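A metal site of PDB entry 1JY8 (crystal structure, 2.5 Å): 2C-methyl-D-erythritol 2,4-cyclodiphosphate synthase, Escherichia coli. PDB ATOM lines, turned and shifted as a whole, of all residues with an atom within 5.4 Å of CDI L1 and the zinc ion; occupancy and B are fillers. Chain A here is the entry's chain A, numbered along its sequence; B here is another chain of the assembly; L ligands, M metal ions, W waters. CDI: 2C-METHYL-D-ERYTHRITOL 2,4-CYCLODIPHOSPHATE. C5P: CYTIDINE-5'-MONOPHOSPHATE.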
ATOM      1  N   ASP A   8      14.542  10.718  19.012  1.00  0.00           N
ATOM      2  CA  ASP A   8      15.653  11.675  19.079  1.00  0.00           C
ATOM      3  C   ASP A   8      15.301  12.864  19.983  1.00  0.00           C
ATOM      4  O   ASP A   8      14.113  13.158  20.228  1.00  0.00           O
ATOM      5  CB  ASP A   8      16.015  12.163  17.678  1.00  0.00           C
ATOM      6  CG  ASP A   8      17.368  12.859  17.634  1.00  0.00           C
ATOM      7  OD1 ASP A   8      17.580  13.658  16.704  1.00  0.00           O
ATOM      8  OD2 ASP A   8      18.226  12.640  18.523  1.00  0.00           O
ATOM      9  N   VAL A   9      16.344  13.514  20.509  1.00  0.00           N
ATOM     10  CA  VAL A   9      16.209  14.672  21.395  1.00  0.00           C
ATOM     11  C   VAL A   9      17.344  15.660  21.117  1.00  0.00           C
ATOM     12  O   VAL A   9      18.463  15.244  20.779  1.00  0.00           O
ATOM     13  CB  VAL A   9      16.305  14.258  22.906  1.00  0.00           C
ATOM     14  CG1 VAL A   9      16.413  15.475  23.795  1.00  0.00           C
ATOM     15  CG2 VAL A   9      15.100  13.458  23.328  1.00  0.00           C
ATOM     16  N   HIS A  10      17.024  16.956  21.165  1.00  0.00           N
ATOM     17  CA  HIS A  10      18.010  18.030  20.987  1.00  0.00           C
ATOM     18  C   HIS A  10      17.668  19.146  21.959  1.00  0.00           C
ATOM     19  O   HIS A  10      16.504  19.420  22.232  1.00  0.00           O
ATOM     20  CB  HIS A  10      18.113  18.518  19.546  1.00  0.00           C
ATOM     21  CG  HIS A  10      18.891  17.583  18.673  1.00  0.00           C
ATOM     22  ND1 HIS A  10      20.227  17.315  18.882  1.00  0.00           N
ATOM     23  CD2 HIS A  10      18.495  16.766  17.665  1.00  0.00           C
ATOM     24  CE1 HIS A  10      20.614  16.369  18.046  1.00  0.00           C
ATOM     25  NE2 HIS A  10      19.579  16.012  17.301  1.00  0.00           N
ATOM     26  N   ALA A  33      23.083  21.039  17.993  1.00  0.00           N
ATOM     27  CA  ALA A  33      23.376  19.749  17.357  1.00  0.00           C
ATOM     28  C   ALA A  33      24.536  19.864  16.370  1.00  0.00           C
ATOM     29  O   ALA A  33      24.928  20.971  16.010  1.00  0.00           O
ATOM     30  CB  ALA A  33      22.129  19.224  16.642  1.00  0.00           C
ATOM     31  N   HIS A  34      25.103  18.719  15.978  1.00  0.00           N
ATOM     32  CA  HIS A  34      26.208  18.673  15.006  1.00  0.00           C
ATOM     33  C   HIS A  34      25.715  19.201  13.659  1.00  0.00           C
ATOM     34  O   HIS A  34      26.385  20.015  13.014  1.00  0.00           O
ATOM     35  CB  HIS A  34      26.722  17.237  14.850  1.00  0.00           C
ATOM     36  CG  HIS A  34      27.928  17.111  13.966  1.00  0.00           C
ATOM     37  ND1 HIS A  34      29.036  17.931  14.078  1.00  0.00           N
ATOM     38  CD2 HIS A  34      28.223  16.223  12.978  1.00  0.00           C
ATOM     39  CE1 HIS A  34      29.955  17.559  13.200  1.00  0.00           C
ATOM     40  NE2 HIS A  34      29.484  16.524  12.525  1.00  0.00           N
ATOM     41  N   SER A  35      24.572  18.681  13.211  1.00  0.00           N
ATOM     42  CA  SER A  35      23.928  19.065  11.958  1.00  0.00           C
ATOM     43  C   SER A  35      23.013  20.237  12.309  1.00  0.00           C
ATOM     44  O   SER A  35      23.243  20.928  13.298  1.00  0.00           O
ATOM     45  CB  SER A  35      23.085  17.890  11.432  1.00  0.00           C
ATOM     46  OG  SER A  35      21.953  17.636  12.247  1.00  0.00           O
ATOM     47  N   ASP A  36      21.956  20.445  11.524  1.00  0.00           N
ATOM     48  CA  ASP A  36      21.000  21.516  11.792  1.00  0.00           C
ATOM     49  C   ASP A  36      20.110  21.175  13.011  1.00  0.00           C
ATOM     50  O   ASP A  36      19.245  21.965  13.381  1.00  0.00           O
ATOM     51  CB  ASP A  36      20.121  21.787  10.567  1.00  0.00           C
ATOM     52  CG  ASP A  36      19.396  20.554  10.091  1.00  0.00           C
ATOM     53  OD1 ASP A  36      18.750  20.630   9.027  1.00  0.00           O
ATOM     54  OD2 ASP A  36      19.468  19.506  10.762  1.00  0.00           O
ATOM     55  N   GLY A  37      20.295  19.978  13.567  1.00  0.00           N
ATOM     56  CA  GLY A  37      19.560  19.553  14.741  1.00  0.00           C
ATOM     57  C   GLY A  37      18.092  19.224  14.560  1.00  0.00           C
ATOM     58  O   GLY A  37      17.343  19.181  15.541  1.00  0.00           O
ATOM     59  N   ASP A  38      17.686  18.937  13.334  1.00  0.00           N
ATOM     60  CA  ASP A  38      16.297  18.607  13.053  1.00  0.00           C
ATOM     61  C   ASP A  38      15.885  17.302  13.755  1.00  0.00           C
ATOM     62  O   ASP A  38      16.085  16.207  13.230  1.00  0.00           O
ATOM     63  CB  ASP A  38      16.099  18.496  11.549  1.00  0.00           C
ATOM     64  CG  ASP A  38      14.668  18.544  11.134  1.00  0.00           C
ATOM     65  OD1 ASP A  38      13.824  17.943  11.832  1.00  0.00           O
ATOM     66  OD2 ASP A  38      14.380  19.157  10.098  1.00  0.00           O
ATOM     67  N   VAL A  39      15.301  17.427  14.939  1.00  0.00           N
ATOM     68  CA  VAL A  39      14.892  16.273  15.738  1.00  0.00           C
ATOM     69  C   VAL A  39      13.902  15.351  15.024  1.00  0.00           C
ATOM     70  O   VAL A  39      13.946  14.133  15.210  1.00  0.00           O
ATOM     71  CB  VAL A  39      14.219  16.681  17.061  1.00  0.00           C
ATOM     72  CG1 VAL A  39      14.434  15.607  18.097  1.00  0.00           C
ATOM     73  CG2 VAL A  39      14.755  17.976  17.550  1.00  0.00           C
ATOM     74  N   HIS A  42      15.688  13.307  12.124  1.00  0.00           N
ATOM     75  CA  HIS A  42      16.631  12.336  12.675  1.00  0.00           C
ATOM     76  C   HIS A  42      15.828  11.124  13.151  1.00  0.00           C
ATOM     77  O   HIS A  42      16.124   9.993  12.796  1.00  0.00           O
ATOM     78  CB  HIS A  42      17.401  12.888  13.866  1.00  0.00           C
ATOM     79  CG  HIS A  42      18.400  13.948  13.503  1.00  0.00           C
ATOM     80  ND1 HIS A  42      19.201  14.570  14.444  1.00  0.00           N
ATOM     81  CD2 HIS A  42      18.726  14.484  12.309  1.00  0.00           C
ATOM     82  CE1 HIS A  42      19.974  15.452  13.836  1.00  0.00           C
ATOM     83  NE2 HIS A  42      19.710  15.425  12.538  1.00  0.00           N
ATOM     84  N   ILE A  57      21.263   6.507  12.421  1.00  0.00           N
ATOM     85  CA  ILE A  57      21.844   7.719  11.852  1.00  0.00           C
ATOM     86  C   ILE A  57      23.280   7.997  12.260  1.00  0.00           C
ATOM     87  O   ILE A  57      24.094   8.377  11.423  1.00  0.00           O
ATOM     88  CB  ILE A  57      20.923   8.953  12.143  1.00  0.00           C
ATOM     89  CG1 ILE A  57      21.203  10.068  11.166  1.00  0.00           C
ATOM     90  CG2 ILE A  57      21.118   9.472  13.558  1.00  0.00           C
ATOM     91  CD1 ILE A  57      20.262  11.222  11.342  1.00  0.00           C
ATOM     92  N   GLY A  58      23.607   7.753  13.526  1.00  0.00           N
ATOM     93  CA  GLY A  58      24.966   8.006  13.992  1.00  0.00           C
ATOM     94  C   GLY A  58      25.984   7.090  13.367  1.00  0.00           C
ATOM     95  O   GLY A  58      27.130   7.471  13.111  1.00  0.00           O
ATOM     96  N   PHE A  61      26.262   8.498   9.661  1.00  0.00           N
ATOM     97  CA  PHE A  61      26.756   9.863   9.588  1.00  0.00           C
ATOM     98  C   PHE A  61      27.275  10.314  10.964  1.00  0.00           C
ATOM     99  O   PHE A  61      26.620  11.078  11.659  1.00  0.00           O
ATOM    100  CB  PHE A  61      25.636  10.810   9.111  1.00  0.00           C
ATOM    101  CG  PHE A  61      24.780  10.228   8.001  1.00  0.00           C
ATOM    102  CD1 PHE A  61      25.313   9.944   6.754  1.00  0.00           C
ATOM    103  CD2 PHE A  61      23.428   9.944   8.227  1.00  0.00           C
ATOM    104  CE1 PHE A  61      24.527   9.364   5.752  1.00  0.00           C
ATOM    105  CE2 PHE A  61      22.637   9.367   7.232  1.00  0.00           C
ATOM    106  CZ  PHE A  61      23.189   9.075   5.991  1.00  0.00           C
ATOM    107  N   PRO A  62      28.484   9.877  11.338  1.00  0.00           N
ATOM    108  CA  PRO A  62      29.170  10.177  12.601  1.00  0.00           C
ATOM    109  C   PRO A  62      29.275  11.637  13.070  1.00  0.00           C
ATOM    110  O   PRO A  62      29.673  12.516  12.317  1.00  0.00           O
ATOM    111  CB  PRO A  62      30.559   9.588  12.363  1.00  0.00           C
ATOM    112  CG  PRO A  62      30.272   8.419  11.502  1.00  0.00           C
ATOM    113  CD  PRO A  62      29.324   9.007  10.498  1.00  0.00           C
ATOM    114  N   ASP A  63      28.991  11.828  14.364  1.00  0.00           N
ATOM    115  CA  ASP A  63      29.065  13.136  15.037  1.00  0.00           C
ATOM    116  C   ASP A  63      30.457  13.721  14.924  1.00  0.00           C
ATOM    117  O   ASP A  63      30.645  14.938  14.973  1.00  0.00           O
ATOM    118  CB  ASP A  63      28.757  12.964  16.541  1.00  0.00           C
ATOM    119  CG  ASP A  63      27.306  13.229  16.876  1.00  0.00           C
ATOM    120  OD1 ASP A  63      26.429  13.106  15.988  1.00  0.00           O
ATOM    121  OD2 ASP A  63      27.025  13.581  18.046  1.00  0.00           O
ATOM    122  N   ASP A  65      32.714  13.100  12.298  1.00  0.00           N
ATOM    123  CA  ASP A  65      33.008  13.501  10.937  1.00  0.00           C
ATOM    124  C   ASP A  65      32.515  14.933  10.707  1.00  0.00           C
ATOM    125  O   ASP A  65      31.304  15.189  10.708  1.00  0.00           O
ATOM    126  CB  ASP A  65      32.342  12.541   9.955  1.00  0.00           C
ATOM    127  CG  ASP A  65      32.849  12.712   8.540  1.00  0.00           C
ATOM    128  OD1 ASP A  65      33.255  13.834   8.170  1.00  0.00           O
ATOM    129  OD2 ASP A  65      32.849  11.703   7.792  1.00  0.00           O
ATOM    130  N   PHE A  68      29.623  16.465   8.355  1.00  0.00           N
ATOM    131  CA  PHE A  68      28.223  16.558   8.739  1.00  0.00           C
ATOM    132  C   PHE A  68      27.928  17.735   9.652  1.00  0.00           C
ATOM    133  O   PHE A  68      26.877  17.777  10.278  1.00  0.00           O
ATOM    134  CB  PHE A  68      27.797  15.245   9.407  1.00  0.00           C
ATOM    135  CG  PHE A  68      28.273  14.030   8.679  1.00  0.00           C
ATOM    136  CD1 PHE A  68      29.040  13.068   9.317  1.00  0.00           C
ATOM    137  CD2 PHE A  68      27.976  13.847   7.330  1.00  0.00           C
ATOM    138  CE1 PHE A  68      29.498  11.943   8.641  1.00  0.00           C
ATOM    139  CE2 PHE A  68      28.419  12.727   6.641  1.00  0.00           C
ATOM    140  CZ  PHE A  68      29.191  11.775   7.292  1.00  0.00           C
ATOM    141  N   SER A  73      19.662  18.027   7.536  1.00  0.00           N
ATOM    142  CA  SER A  73      19.124  16.718   7.872  1.00  0.00           C
ATOM    143  C   SER A  73      18.307  16.084   6.748  1.00  0.00           C
ATOM    144  O   SER A  73      18.088  14.876   6.751  1.00  0.00           O
ATOM    145  CB  SER A  73      18.330  16.771   9.164  1.00  0.00           C
ATOM    146  OG  SER A  73      19.183  16.982  10.276  1.00  0.00           O
ATOM    147  N   LEU A  76      20.702  14.111   4.791  1.00  0.00           N
ATOM    148  CA  LEU A  76      20.950  12.845   5.481  1.00  0.00           C
ATOM    149  C   LEU A  76      19.778  11.892   5.298  1.00  0.00           C
ATOM    150  O   LEU A  76      19.957  10.692   5.164  1.00  0.00           O
ATOM    151  CB  LEU A  76      21.190  13.089   6.973  1.00  0.00           C
ATOM    152  CG  LEU A  76      22.363  13.977   7.388  1.00  0.00           C
ATOM    153  CD1 LEU A  76      22.504  13.940   8.914  1.00  0.00           C
ATOM    154  CD2 LEU A  76      23.645  13.481   6.741  1.00  0.00           C
ATOM    155  N   THR B 132      20.625   6.211  21.176  1.00  0.00           N
ATOM    156  CA  THR B 132      20.594   7.666  21.109  1.00  0.00           C
ATOM    157  C   THR B 132      20.673   8.183  22.543  1.00  0.00           C
ATOM    158  O   THR B 132      20.340   7.459  23.479  1.00  0.00           O
ATOM    159  CB  THR B 132      19.321   8.210  20.436  1.00  0.00           C
ATOM    160  OG1 THR B 132      19.476   9.620  20.199  1.00  0.00           O
ATOM    161  CG2 THR B 132      18.092   8.006  21.329  1.00  0.00           C
ATOM    162  N   GLU B 135      20.761  14.078  24.912  1.00  0.00           N
ATOM    163  CA  GLU B 135      21.586  15.293  25.003  1.00  0.00           C
ATOM    164  C   GLU B 135      21.681  15.900  26.408  1.00  0.00           C
ATOM    165  O   GLU B 135      21.449  17.095  26.596  1.00  0.00           O
ATOM    166  CB  GLU B 135      21.081  16.335  24.010  1.00  0.00           C
ATOM    167  CG  GLU B 135      20.865  15.824  22.588  1.00  0.00           C
ATOM    168  CD  GLU B 135      22.149  15.651  21.786  1.00  0.00           C
ATOM    169  OE1 GLU B 135      22.101  15.108  20.672  1.00  0.00           O
ATOM    170  OE2 GLU B 135      23.217  16.087  22.267  1.00  0.00           O
HETATM  171  C4  CDI L   1      25.153  14.128  12.248  1.00  0.00           C
HETATM  172  C3  CDI L   1      24.118  13.556  13.267  1.00  0.00           C
HETATM  173  OB4 CDI L   1      24.240  14.319  14.503  1.00  0.00           O
HETATM  174  PB  CDI L   1      23.447  15.427  15.394  1.00  0.00           P
HETATM  175  OB2 CDI L   1      24.270  15.823  16.682  1.00  0.00           O
HETATM  176  OB3 CDI L   1      23.095  16.743  14.533  1.00  0.00           O
HETATM  177  PA  CDI L   1      22.409  13.355  16.742  1.00  0.00           P
HETATM  178  OA3 CDI L   1      23.265  12.193  16.018  1.00  0.00           O
HETATM  179  OA1 CDI L   1      22.904  13.617  18.210  1.00  0.00           O
HETATM  180  OA2 CDI L   1      20.845  13.044  16.760  1.00  0.00           O
HETATM  181  C1  CDI L   1      23.368  11.470  14.752  1.00  0.00           C
HETATM  182  C2  CDI L   1      24.375  12.071  13.685  1.00  0.00           C
HETATM  183  O1  CDI L   1      24.280  11.197  12.560  1.00  0.00           O
HETATM  184  C5  CDI L   1      22.699  13.697  12.632  1.00  0.00           C
HETATM  185  O2  CDI L   1      26.494  14.020  12.767  1.00  0.00           O
HETATM  186  OB1 CDI L   1      22.334  14.773  16.240  1.00  0.00           O
HETATM  187  O3P C5P L   2      22.287  11.312  18.659  1.00  0.00           O
HETATM  188  P   C5P L   2      23.563  10.954  19.668  1.00  0.00           P
HETATM  189  O1P C5P L   2      23.029  10.505  21.025  1.00  0.00           O
HETATM  190  O2P C5P L   2      24.487  12.169  19.850  1.00  0.00           O
HETATM  191  O5' C5P L   2      24.498   9.733  19.020  1.00  0.00           O
HETATM  192  C5' C5P L   2      24.057   8.948  17.921  1.00  0.00           C
HETATM  193  C4' C5P L   2      24.970   7.798  17.775  1.00  0.00           C
HETATM  194  O4' C5P L   2      25.732   7.517  18.940  1.00  0.00           O
HETATM  195  C3' C5P L   2      24.002   6.610  17.666  1.00  0.00           C
HETATM  196  O3' C5P L   2      24.394   5.947  16.506  1.00  0.00           O
HETATM  197  C2' C5P L   2      24.272   5.725  18.864  1.00  0.00           C
HETATM  198  O2' C5P L   2      24.365   4.318  18.580  1.00  0.00           O
HETATM  199  C1' C5P L   2      25.589   6.209  19.369  1.00  0.00           C
HETATM  200  N1  C5P L   2      25.120   6.209  20.685  1.00  0.00           N
HETATM  201  C2  C5P L   2      25.591   5.062  21.361  1.00  0.00           C
HETATM  202  N3  C5P L   2      25.319   4.823  22.681  1.00  0.00           N
HETATM  203  C4  C5P L   2      24.579   5.691  23.384  1.00  0.00           C
HETATM  204  C5  C5P L   2      24.079   6.834  22.767  1.00  0.00           C
HETATM  205  C6  C5P L   2      24.381   7.037  21.432  1.00  0.00           C
HETATM  206  O2  C5P L   2      26.295   4.194  20.818  1.00  0.00           O
HETATM  207  N4  C5P L   2      24.336   5.435  24.667  1.00  0.00           N
HETATM  208 ZN    ZN M   1      19.384  14.272  16.389  1.00  0.00          ZN
HETATM  209  O   HOH W   1      20.516  13.006  20.555  1.00  0.00           O
HETATM  210  O   HOH W   2      23.765  16.509  19.090  1.00  0.00           O
HETATM  211  O   HOH W   3      27.118  16.456  17.929  1.00  0.00           O
HETATM  212  O   HOH W   4      19.955  10.188  17.510  1.00  0.00           O
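O of Phe 61 sits at hydrogen-bond distance from O1 of CDI L1 (2.5 Å). N of Ser 35 sits at hydrogen-bond distance from OB3 of CDI L1, 2.8 Å away. The side-chain hydroxyl of Ser 35 is in hydrogen-bond range of an oxygen (OB3) of CDI L1 (2.7 Å). OB2 of CDI L1 lies within hydrogen-bond range of N of His 34 (3.1 Å). The side-chain carboxylate of Asp 63 lies close to an oxygen (O2) of CDI L1 (3.3 Å). OE1 of Glu 135 of chain B lies close to OA1 of CDI L1. O of Ile 57 sits at hydrogen-bond distance from O1 of CDI L1, 3.0 Å away.
An oxygen (OA2) of CDI L1 lies close to an oxygen (O3P) of C5P L2, 2.9 Å away.
A ring nitrogen (ND1) of His 10 sits close to the side-chain carboxylate (OE1) of Glu 135 of chain B, 3.4 Å away. NE2 of His 42 sits at hydrogen-bond distance from OG of Ser 35 (3.2 Å). The side-chain hydroxyl (OG) of Ser 73 lies within hydrogen-bond range of a ring nitrogen (NE2) of His 42 (2.8 Å). N of Gly 37 lies close to OG of Ser 35, 3.2 Å away. The side-chain hydroxyl (OG) of Ser 35 lies within hydrogen-bond range of the side-chain carboxylate (OD2) of Asp 36. OG of Ser 73 lies within hydrogen-bond range of OG of Ser 35 (3.5 Å). A ring nitrogen (NE2) of His 34 lies within hydrogen-bond range of the backbone carbonyl oxygen (O) of Asp 63. A ring nitrogen (NE2) of His 34 sits at hydrogen-bond distance from the backbone carbonyl oxygen (O) of Asp 65, 2.9 Å away.
Merely in contact with CDI L1: Ala 33 (3.4 Å), Pro 62 (3.5 Å), Gly 58 (3.6 Å), Leu 76 (3.7 Å) and Phe 68 (3.8 Å). Of the 22 residues printed, 14 come within 4 Å of CDI L1. The nearest printed residue that does not touch CDI L1 is Gly 37 (4.4 Å).
Of the 22 residues printed, 3 come within 4 Å of the zinc ion.
The zinc ion is bound by the side-chain carboxylate of Asp 8 (1.9 Å), an oxygen (OA2) of CDI L1 (1.9 Å), a ring nitrogen (NE2) of His 10 (2.0 Å) and a ring nitrogen (ND1) of His 42 (2.0 Å).
Water W2 bridges an oxygen (OB2) of CDI L1 (2.6 Å) and the side-chain carboxylate of Glu 135 of chain B (2.7 Å). Water W4 lies within hydrogen-bond range of OG1 of Thr 132 of chain B (2.8 Å), O3P of C5P L2 (2.8 Å) and OD2 of Asp 8 (3.2 Å). Water W3 bridges the side-chain carboxylate of Asp 63 and an oxygen (OB2) of CDI L1.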
